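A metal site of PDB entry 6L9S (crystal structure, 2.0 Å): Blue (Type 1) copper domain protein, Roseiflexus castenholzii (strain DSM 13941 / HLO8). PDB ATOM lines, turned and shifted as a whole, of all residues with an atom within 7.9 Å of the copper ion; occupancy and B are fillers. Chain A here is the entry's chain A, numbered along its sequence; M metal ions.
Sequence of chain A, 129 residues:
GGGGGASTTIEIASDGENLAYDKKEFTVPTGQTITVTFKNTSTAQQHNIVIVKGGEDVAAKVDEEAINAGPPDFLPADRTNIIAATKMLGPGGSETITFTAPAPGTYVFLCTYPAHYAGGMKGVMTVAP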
ATOM      1  N   SER A  14      -6.967 -15.239  16.596  1.00  0.00           N
ATOM      2  CA  SER A  14      -5.921 -14.579  15.856  1.00  0.00           C
ATOM      3  C   SER A  14      -6.348 -14.451  14.395  1.00  0.00           C
ATOM      4  O   SER A  14      -7.102 -15.277  13.896  1.00  0.00           O
ATOM      5  CB  SER A  14      -4.612 -15.312  15.980  1.00  0.00           C
ATOM      6  OG  SER A  14      -4.751 -16.663  15.555  1.00  0.00           O
ATOM      7  N   ASN A  18      -1.140 -13.012  11.215  1.00  0.00           N
ATOM      8  CA  ASN A  18      -0.923 -11.592  11.512  1.00  0.00           C
ATOM      9  C   ASN A  18      -0.976 -11.353  13.028  1.00  0.00           C
ATOM     10  O   ASN A  18      -1.563 -12.146  13.768  1.00  0.00           O
ATOM     11  CB  ASN A  18      -1.927 -10.708  10.775  1.00  0.00           C
ATOM     12  CG  ASN A  18      -1.795 -10.806   9.273  1.00  0.00           C
ATOM     13  OD1 ASN A  18      -0.684 -10.851   8.734  1.00  0.00           O
ATOM     14  ND2 ASN A  18      -2.917 -10.848   8.569  1.00  0.00           N
ATOM     15  N   LEU A  19      -0.363 -10.251  13.460  1.00  0.00           N
ATOM     16  CA  LEU A  19      -0.388  -9.814  14.856  1.00  0.00           C
ATOM     17  C   LEU A  19      -1.646  -8.972  15.086  1.00  0.00           C
ATOM     18  O   LEU A  19      -1.585  -7.752  15.239  1.00  0.00           O
ATOM     19  CB  LEU A  19       0.880  -9.009  15.144  1.00  0.00           C
ATOM     20  CG  LEU A  19       2.205  -9.768  14.988  1.00  0.00           C
ATOM     21  CD1 LEU A  19       3.373  -8.915  15.463  1.00  0.00           C
ATOM     22  CD2 LEU A  19       2.174 -11.089  15.738  1.00  0.00           C
ATOM     23  N   ALA A  20      -2.789  -9.665  15.080  1.00  0.00           N
ATOM     24  CA  ALA A  20      -4.091  -9.051  15.249  1.00  0.00           C
ATOM     25  C   ALA A  20      -5.099 -10.129  15.641  1.00  0.00           C
ATOM     26  O   ALA A  20      -4.877 -11.315  15.396  1.00  0.00           O
ATOM     27  CB  ALA A  20      -4.511  -8.335  13.983  1.00  0.00           C
ATOM     28  N   TYR A  21      -6.206  -9.684  16.260  1.00  0.00           N
ATOM     29  CA  TYR A  21      -7.388 -10.507  16.498  1.00  0.00           C
ATOM     30  C   TYR A  21      -8.348 -10.292  15.329  1.00  0.00           C
ATOM     31  O   TYR A  21      -8.186  -9.346  14.548  1.00  0.00           O
ATOM     32  CB  TYR A  21      -8.041 -10.134  17.831  1.00  0.00           C
ATOM     33  CG  TYR A  21      -7.179 -10.353  19.047  1.00  0.00           C
ATOM     34  CD1 TYR A  21      -7.032 -11.618  19.598  1.00  0.00           C
ATOM     35  CD2 TYR A  21      -6.525  -9.307  19.672  1.00  0.00           C
ATOM     36  CE1 TYR A  21      -6.241 -11.835  20.722  1.00  0.00           C
ATOM     37  CE2 TYR A  21      -5.726  -9.506  20.786  1.00  0.00           C
ATOM     38  CZ  TYR A  21      -5.592 -10.776  21.318  1.00  0.00           C
ATOM     39  OH  TYR A  21      -4.823 -10.980  22.432  1.00  0.00           O
ATOM     40  N   PHE A  38     -10.929 -18.025  23.096  1.00  0.00           N
ATOM     41  CA  PHE A  38      -9.881 -17.547  22.218  1.00  0.00           C
ATOM     42  C   PHE A  38      -9.222 -18.738  21.503  1.00  0.00           C
ATOM     43  O   PHE A  38      -8.810 -19.699  22.161  1.00  0.00           O
ATOM     44  CB  PHE A  38      -8.834 -16.731  22.982  1.00  0.00           C
ATOM     45  CG  PHE A  38      -7.602 -16.414  22.172  1.00  0.00           C
ATOM     46  CD1 PHE A  38      -7.711 -15.702  20.982  1.00  0.00           C
ATOM     47  CD2 PHE A  38      -6.351 -16.856  22.568  1.00  0.00           C
ATOM     48  CE1 PHE A  38      -6.585 -15.418  20.218  1.00  0.00           C
ATOM     49  CE2 PHE A  38      -5.228 -16.560  21.807  1.00  0.00           C
ATOM     50  CZ  PHE A  38      -5.346 -15.852  20.631  1.00  0.00           C
ATOM     51  N   ASN A  40      -6.075 -19.684  18.916  1.00  0.00           N
ATOM     52  CA  ASN A  40      -4.858 -19.398  18.172  1.00  0.00           C
ATOM     53  C   ASN A  40      -4.921 -20.178  16.844  1.00  0.00           C
ATOM     54  O   ASN A  40      -4.686 -21.377  16.808  1.00  0.00           O
ATOM     55  CB  ASN A  40      -3.618 -19.734  18.988  1.00  0.00           C
ATOM     56  CG  ASN A  40      -2.311 -19.445  18.264  1.00  0.00           C
ATOM     57  OD1 ASN A  40      -2.314 -19.087  17.099  1.00  0.00           O
ATOM     58  ND2 ASN A  40      -1.196 -19.614  18.959  1.00  0.00           N
ATOM     59  N   GLN A  45       2.860 -19.536  15.610  1.00  0.00           N
ATOM     60  CA  GLN A  45       3.009 -18.452  16.573  1.00  0.00           C
ATOM     61  C   GLN A  45       2.277 -18.773  17.873  1.00  0.00           C
ATOM     62  O   GLN A  45       1.322 -19.550  17.891  1.00  0.00           O
ATOM     63  CB  GLN A  45       2.487 -17.137  15.990  1.00  0.00           C
ATOM     64  CG  GLN A  45       3.107 -16.808  14.636  1.00  0.00           C
ATOM     65  CD  GLN A  45       2.998 -15.343  14.308  1.00  0.00           C
ATOM     66  OE1 GLN A  45       3.384 -14.490  15.091  1.00  0.00           O
ATOM     67  NE2 GLN A  45       2.479 -15.057  13.133  1.00  0.00           N
ATOM     68  N   GLN A  46       2.742 -18.157  18.968  1.00  0.00           N
ATOM     69  CA  GLN A  46       2.136 -18.271  20.285  1.00  0.00           C
ATOM     70  C   GLN A  46       1.387 -16.976  20.585  1.00  0.00           C
ATOM     71  O   GLN A  46       1.915 -15.880  20.368  1.00  0.00           O
ATOM     72  CB  GLN A  46       3.190 -18.571  21.340  1.00  0.00           C
ATOM     73  CG  GLN A  46       3.844 -19.936  21.162  1.00  0.00           C
ATOM     74  CD  GLN A  46       4.930 -20.151  22.186  1.00  0.00           C
ATOM     75  OE1 GLN A  46       6.109 -20.062  21.891  1.00  0.00           O
ATOM     76  NE2 GLN A  46       4.514 -20.422  23.416  1.00  0.00           N
ATOM     77  N   HIS A  47       0.151 -17.128  21.097  1.00  0.00           N
ATOM     78  CA  HIS A  47      -0.736 -16.028  21.420  1.00  0.00           C
ATOM     79  C   HIS A  47      -1.529 -16.323  22.693  1.00  0.00           C
ATOM     80  O   HIS A  47      -1.836 -17.484  23.000  1.00  0.00           O
ATOM     81  CB  HIS A  47      -1.739 -15.769  20.285  1.00  0.00           C
ATOM     82  CG  HIS A  47      -1.142 -15.360  18.985  1.00  0.00           C
ATOM     83  ND1 HIS A  47      -0.405 -14.202  18.839  1.00  0.00           N
ATOM     84  CD2 HIS A  47      -1.254 -15.896  17.746  1.00  0.00           C
ATOM     85  CE1 HIS A  47      -0.044 -14.079  17.574  1.00  0.00           C
ATOM     86  NE2 HIS A  47      -0.567 -15.097  16.882  1.00  0.00           N
ATOM     87  N   ASN A  48      -1.896 -15.251  23.397  1.00  0.00           N
ATOM     88  CA  ASN A  48      -2.894 -15.303  24.440  1.00  0.00           C
ATOM     89  C   ASN A  48      -3.877 -14.145  24.214  1.00  0.00           C
ATOM     90  O   ASN A  48      -3.796 -13.432  23.200  1.00  0.00           O
ATOM     91  CB  ASN A  48      -2.251 -15.279  25.831  1.00  0.00           C
ATOM     92  CG  ASN A  48      -1.584 -13.957  26.168  1.00  0.00           C
ATOM     93  OD1 ASN A  48      -1.600 -13.016  25.378  1.00  0.00           O
ATOM     94  ND2 ASN A  48      -0.981 -13.879  27.345  1.00  0.00           N
ATOM     95  N   ILE A  49      -4.810 -13.987  25.145  1.00  0.00           N
ATOM     96  CA  ILE A  49      -5.569 -12.771  25.296  1.00  0.00           C
ATOM     97  C   ILE A  49      -5.636 -12.442  26.788  1.00  0.00           C
ATOM     98  O   ILE A  49      -5.935 -13.305  27.624  1.00  0.00           O
ATOM     99  CB  ILE A  49      -6.962 -12.849  24.625  1.00  0.00           C
ATOM    100  CG1 ILE A  49      -7.681 -11.500  24.695  1.00  0.00           C
ATOM    101  CG2 ILE A  49      -7.807 -13.966  25.219  1.00  0.00           C
ATOM    102  CD1 ILE A  49      -8.910 -11.405  23.816  1.00  0.00           C
ATOM    103  N   MET A  88      -0.618 -19.058  27.505  1.00  0.00           N
ATOM    104  CA  MET A  88       0.023 -18.735  26.229  1.00  0.00           C
ATOM    105  C   MET A  88      -0.142 -19.938  25.297  1.00  0.00           C
ATOM    106  O   MET A  88       0.524 -20.966  25.469  1.00  0.00           O
ATOM    107  CB  MET A  88       1.502 -18.388  26.422  1.00  0.00           C
ATOM    108  CG  MET A  88       2.203 -17.911  25.157  1.00  0.00           C
ATOM    109  SD  MET A  88       1.437 -16.456  24.386  1.00  0.00           S
ATOM    110  CE  MET A  88       1.878 -15.171  25.550  1.00  0.00           C
ATOM    111  N   LEU A  89      -1.054 -19.818  24.333  1.00  0.00           N
ATOM    112  CA  LEU A  89      -1.487 -20.932  23.506  1.00  0.00           C
ATOM    113  C   LEU A  89      -0.559 -21.113  22.303  1.00  0.00           C
ATOM    114  O   LEU A  89      -0.136 -20.143  21.674  1.00  0.00           O
ATOM    115  CB  LEU A  89      -2.924 -20.676  23.023  1.00  0.00           C
ATOM    116  CG  LEU A  89      -3.964 -20.468  24.121  1.00  0.00           C
ATOM    117  CD1 LEU A  89      -5.341 -20.263  23.510  1.00  0.00           C
ATOM    118  CD2 LEU A  89      -3.969 -21.642  25.089  1.00  0.00           C
ATOM    119  N   LEU A 110      -5.195  -7.467  24.960  1.00  0.00           N
ATOM    120  CA  LEU A 110      -3.959  -7.565  24.215  1.00  0.00           C
ATOM    121  C   LEU A 110      -3.396  -8.987  24.334  1.00  0.00           C
ATOM    122  O   LEU A 110      -3.747  -9.736  25.250  1.00  0.00           O
ATOM    123  CB  LEU A 110      -2.953  -6.541  24.756  1.00  0.00           C
ATOM    124  CG  LEU A 110      -2.354  -6.836  26.136  1.00  0.00           C
ATOM    125  CD1 LEU A 110      -0.982  -6.208  26.272  1.00  0.00           C
ATOM    126  CD2 LEU A 110      -3.274  -6.357  27.252  1.00  0.00           C
ATOM    127  N   CYS A 111      -2.530  -9.319  23.380  1.00  0.00           N
ATOM    128  CA  CYS A 111      -1.630 -10.456  23.512  1.00  0.00           C
ATOM    129  C   CYS A 111      -0.339  -9.966  24.165  1.00  0.00           C
ATOM    130  O   CYS A 111       0.239  -8.960  23.720  1.00  0.00           O
ATOM    131  CB  CYS A 111      -1.322 -11.084  22.163  1.00  0.00           C
ATOM    132  SG  CYS A 111      -0.142 -12.440  22.294  1.00  0.00           S
ATOM    133  N   THR A 112       0.108 -10.673  25.205  1.00  0.00           N
ATOM    134  CA  THR A 112       1.302 -10.255  25.949  1.00  0.00           C
ATOM    135  C   THR A 112       2.546 -11.016  25.467  1.00  0.00           C
ATOM    136  O   THR A 112       3.595 -10.897  26.101  1.00  0.00           O
ATOM    137  CB  THR A 112       1.140 -10.436  27.464  1.00  0.00           C
ATOM    138  OG1 THR A 112       0.876 -11.818  27.742  1.00  0.00           O
ATOM    139  CG2 THR A 112       0.045  -9.571  28.047  1.00  0.00           C
ATOM    140  N   TYR A 113       2.451 -11.777  24.370  1.00  0.00           N
ATOM    141  CA  TYR A 113       3.667 -12.361  23.795  1.00  0.00           C
ATOM    142  C   TYR A 113       4.573 -11.209  23.357  1.00  0.00           C
ATOM    143  O   TYR A 113       4.089 -10.227  22.816  1.00  0.00           O
ATOM    144  CB  TYR A 113       3.411 -13.334  22.642  1.00  0.00           C
ATOM    145  CG  TYR A 113       4.640 -14.143  22.309  1.00  0.00           C
ATOM    146  CD1 TYR A 113       5.609 -13.648  21.432  1.00  0.00           C
ATOM    147  CD2 TYR A 113       4.910 -15.335  22.953  1.00  0.00           C
ATOM    148  CE1 TYR A 113       6.772 -14.359  21.171  1.00  0.00           C
ATOM    149  CE2 TYR A 113       6.062 -16.063  22.694  1.00  0.00           C
ATOM    150  CZ  TYR A 113       7.003 -15.563  21.807  1.00  0.00           C
ATOM    151  OH  TYR A 113       8.151 -16.264  21.554  1.00  0.00           O
ATOM    152  N   PRO A 114       5.901 -11.255  23.665  1.00  0.00           N
ATOM    153  CA  PRO A 114       6.821 -10.176  23.307  1.00  0.00           C
ATOM    154  C   PRO A 114       6.627  -9.585  21.904  1.00  0.00           C
ATOM    155  O   PRO A 114       6.671 -10.308  20.901  1.00  0.00           O
ATOM    156  CB  PRO A 114       8.184 -10.873  23.437  1.00  0.00           C
ATOM    157  CG  PRO A 114       7.984 -11.805  24.603  1.00  0.00           C
ATOM    158  CD  PRO A 114       6.561 -12.318  24.440  1.00  0.00           C
ATOM    159  N   ALA A 115       6.356  -8.261  21.875  1.00  0.00           N
ATOM    160  CA  ALA A 115       6.263  -7.418  20.667  1.00  0.00           C
ATOM    161  C   ALA A 115       4.870  -7.457  20.024  1.00  0.00           C
ATOM    162  O   ALA A 115       4.618  -6.686  19.103  1.00  0.00           O
ATOM    163  CB  ALA A 115       7.332  -7.792  19.651  1.00  0.00           C
ATOM    164  N   HIS A 116       3.981  -8.329  20.499  1.00  0.00           N
ATOM    165  CA  HIS A 116       2.709  -8.572  19.801  1.00  0.00           C
ATOM    166  C   HIS A 116       1.751  -7.401  20.010  1.00  0.00           C
ATOM    167  O   HIS A 116       1.019  -7.035  19.091  1.00  0.00           O
ATOM    168  CB  HIS A 116       2.121  -9.923  20.207  1.00  0.00           C
ATOM    169  CG  HIS A 116       2.773 -11.071  19.523  1.00  0.00           C
ATOM    170  ND1 HIS A 116       2.119 -12.270  19.308  1.00  0.00           N
ATOM    171  CD2 HIS A 116       3.999 -11.205  18.971  1.00  0.00           C
ATOM    172  CE1 HIS A 116       2.938 -13.114  18.693  1.00  0.00           C
ATOM    173  NE2 HIS A 116       4.091 -12.474  18.471  1.00  0.00           N
ATOM    174  N   TYR A 117       1.775  -6.798  21.218  1.00  0.00           N
ATOM    175  CA  TYR A 117       0.931  -5.653  21.563  1.00  0.00           C
ATOM    176  C   TYR A 117       1.327  -4.435  20.713  1.00  0.00           C
ATOM    177  O   TYR A 117       0.470  -3.844  20.049  1.00  0.00           O
ATOM    178  CB  TYR A 117       1.045  -5.333  23.061  1.00  0.00           C
ATOM    179  CG  TYR A 117       0.301  -4.098  23.512  1.00  0.00           C
ATOM    180  CD1 TYR A 117      -1.050  -3.949  23.250  1.00  0.00           C
ATOM    181  CD2 TYR A 117       0.937  -3.093  24.213  1.00  0.00           C
ATOM    182  CE1 TYR A 117      -1.743  -2.823  23.664  1.00  0.00           C
ATOM    183  CE2 TYR A 117       0.270  -1.959  24.641  1.00  0.00           C
ATOM    184  CZ  TYR A 117      -1.086  -1.820  24.357  1.00  0.00           C
ATOM    185  OH  TYR A 117      -1.773  -0.710  24.778  1.00  0.00           O
ATOM    186  N   MET A 121      -1.664  -6.299  18.140  1.00  0.00           N
ATOM    187  CA  MET A 121      -2.502  -7.370  18.630  1.00  0.00           C
ATOM    188  C   MET A 121      -3.209  -6.907  19.911  1.00  0.00           C
ATOM    189  O   MET A 121      -2.798  -7.212  21.027  1.00  0.00           O
ATOM    190  CB  MET A 121      -1.704  -8.642  18.909  1.00  0.00           C
ATOM    191  CG  MET A 121      -2.589  -9.847  19.062  1.00  0.00           C
ATOM    192  SD  MET A 121      -1.783 -11.316  18.454  1.00  0.00           S
ATOM    193  CE  MET A 121      -3.118 -12.491  18.610  1.00  0.00           C
HETATM  194 CU    CU M   1       0.315 -12.903  20.179  1.00  0.00          CU
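A ring nitrogen (ND1) of His 47 lies close to the side-chain sulfur of Met 121.
The backbone NH of His 47 sits close to the side-chain sulfur of Met 88 (3.6 Å).
O of His 47 lies within hydrogen-bond range of N of Leu 89.
The backbone NH of Met 121 sits at hydrogen-bond distance from the backbone carbonyl oxygen of His 116 (2.9 Å).
The backbone carbonyl oxygen of Met 121 lies within hydrogen-bond range of the backbone NH of Cys 111.
The side-chain amide oxygen (OD1) of Asn 48 sits close to the side-chain sulfur (SG) of Cys 111 (3.5 Å).
The backbone NH (N) of Cys 111 sits at hydrogen-bond distance from the side-chain hydroxyl (OH) of Tyr 21 (3.0 Å).
The backbone NH (N) of Met 121 sits at hydrogen-bond distance from the backbone carbonyl oxygen (O) of Leu 19 (3.2 Å).
Gln 46 touches the copper ion (O to CU, 3.4 Å).
Tyr 113 touches the copper ion (CB to CU, 3.98 Å).
Met 121 touches the copper ion.
Six residues have an atom within 4 Å of the copper ion: Gln 46, His 47, Cys 111, Tyr 113, His 116 and Met 121.
The copper ion is bound by ND1 of His 47 (2.0 Å), ND1 of His 116 (2.1 Å) and SG of Cys 111 (2.2 Å).
The copper ion has three donor atoms within binding distance.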
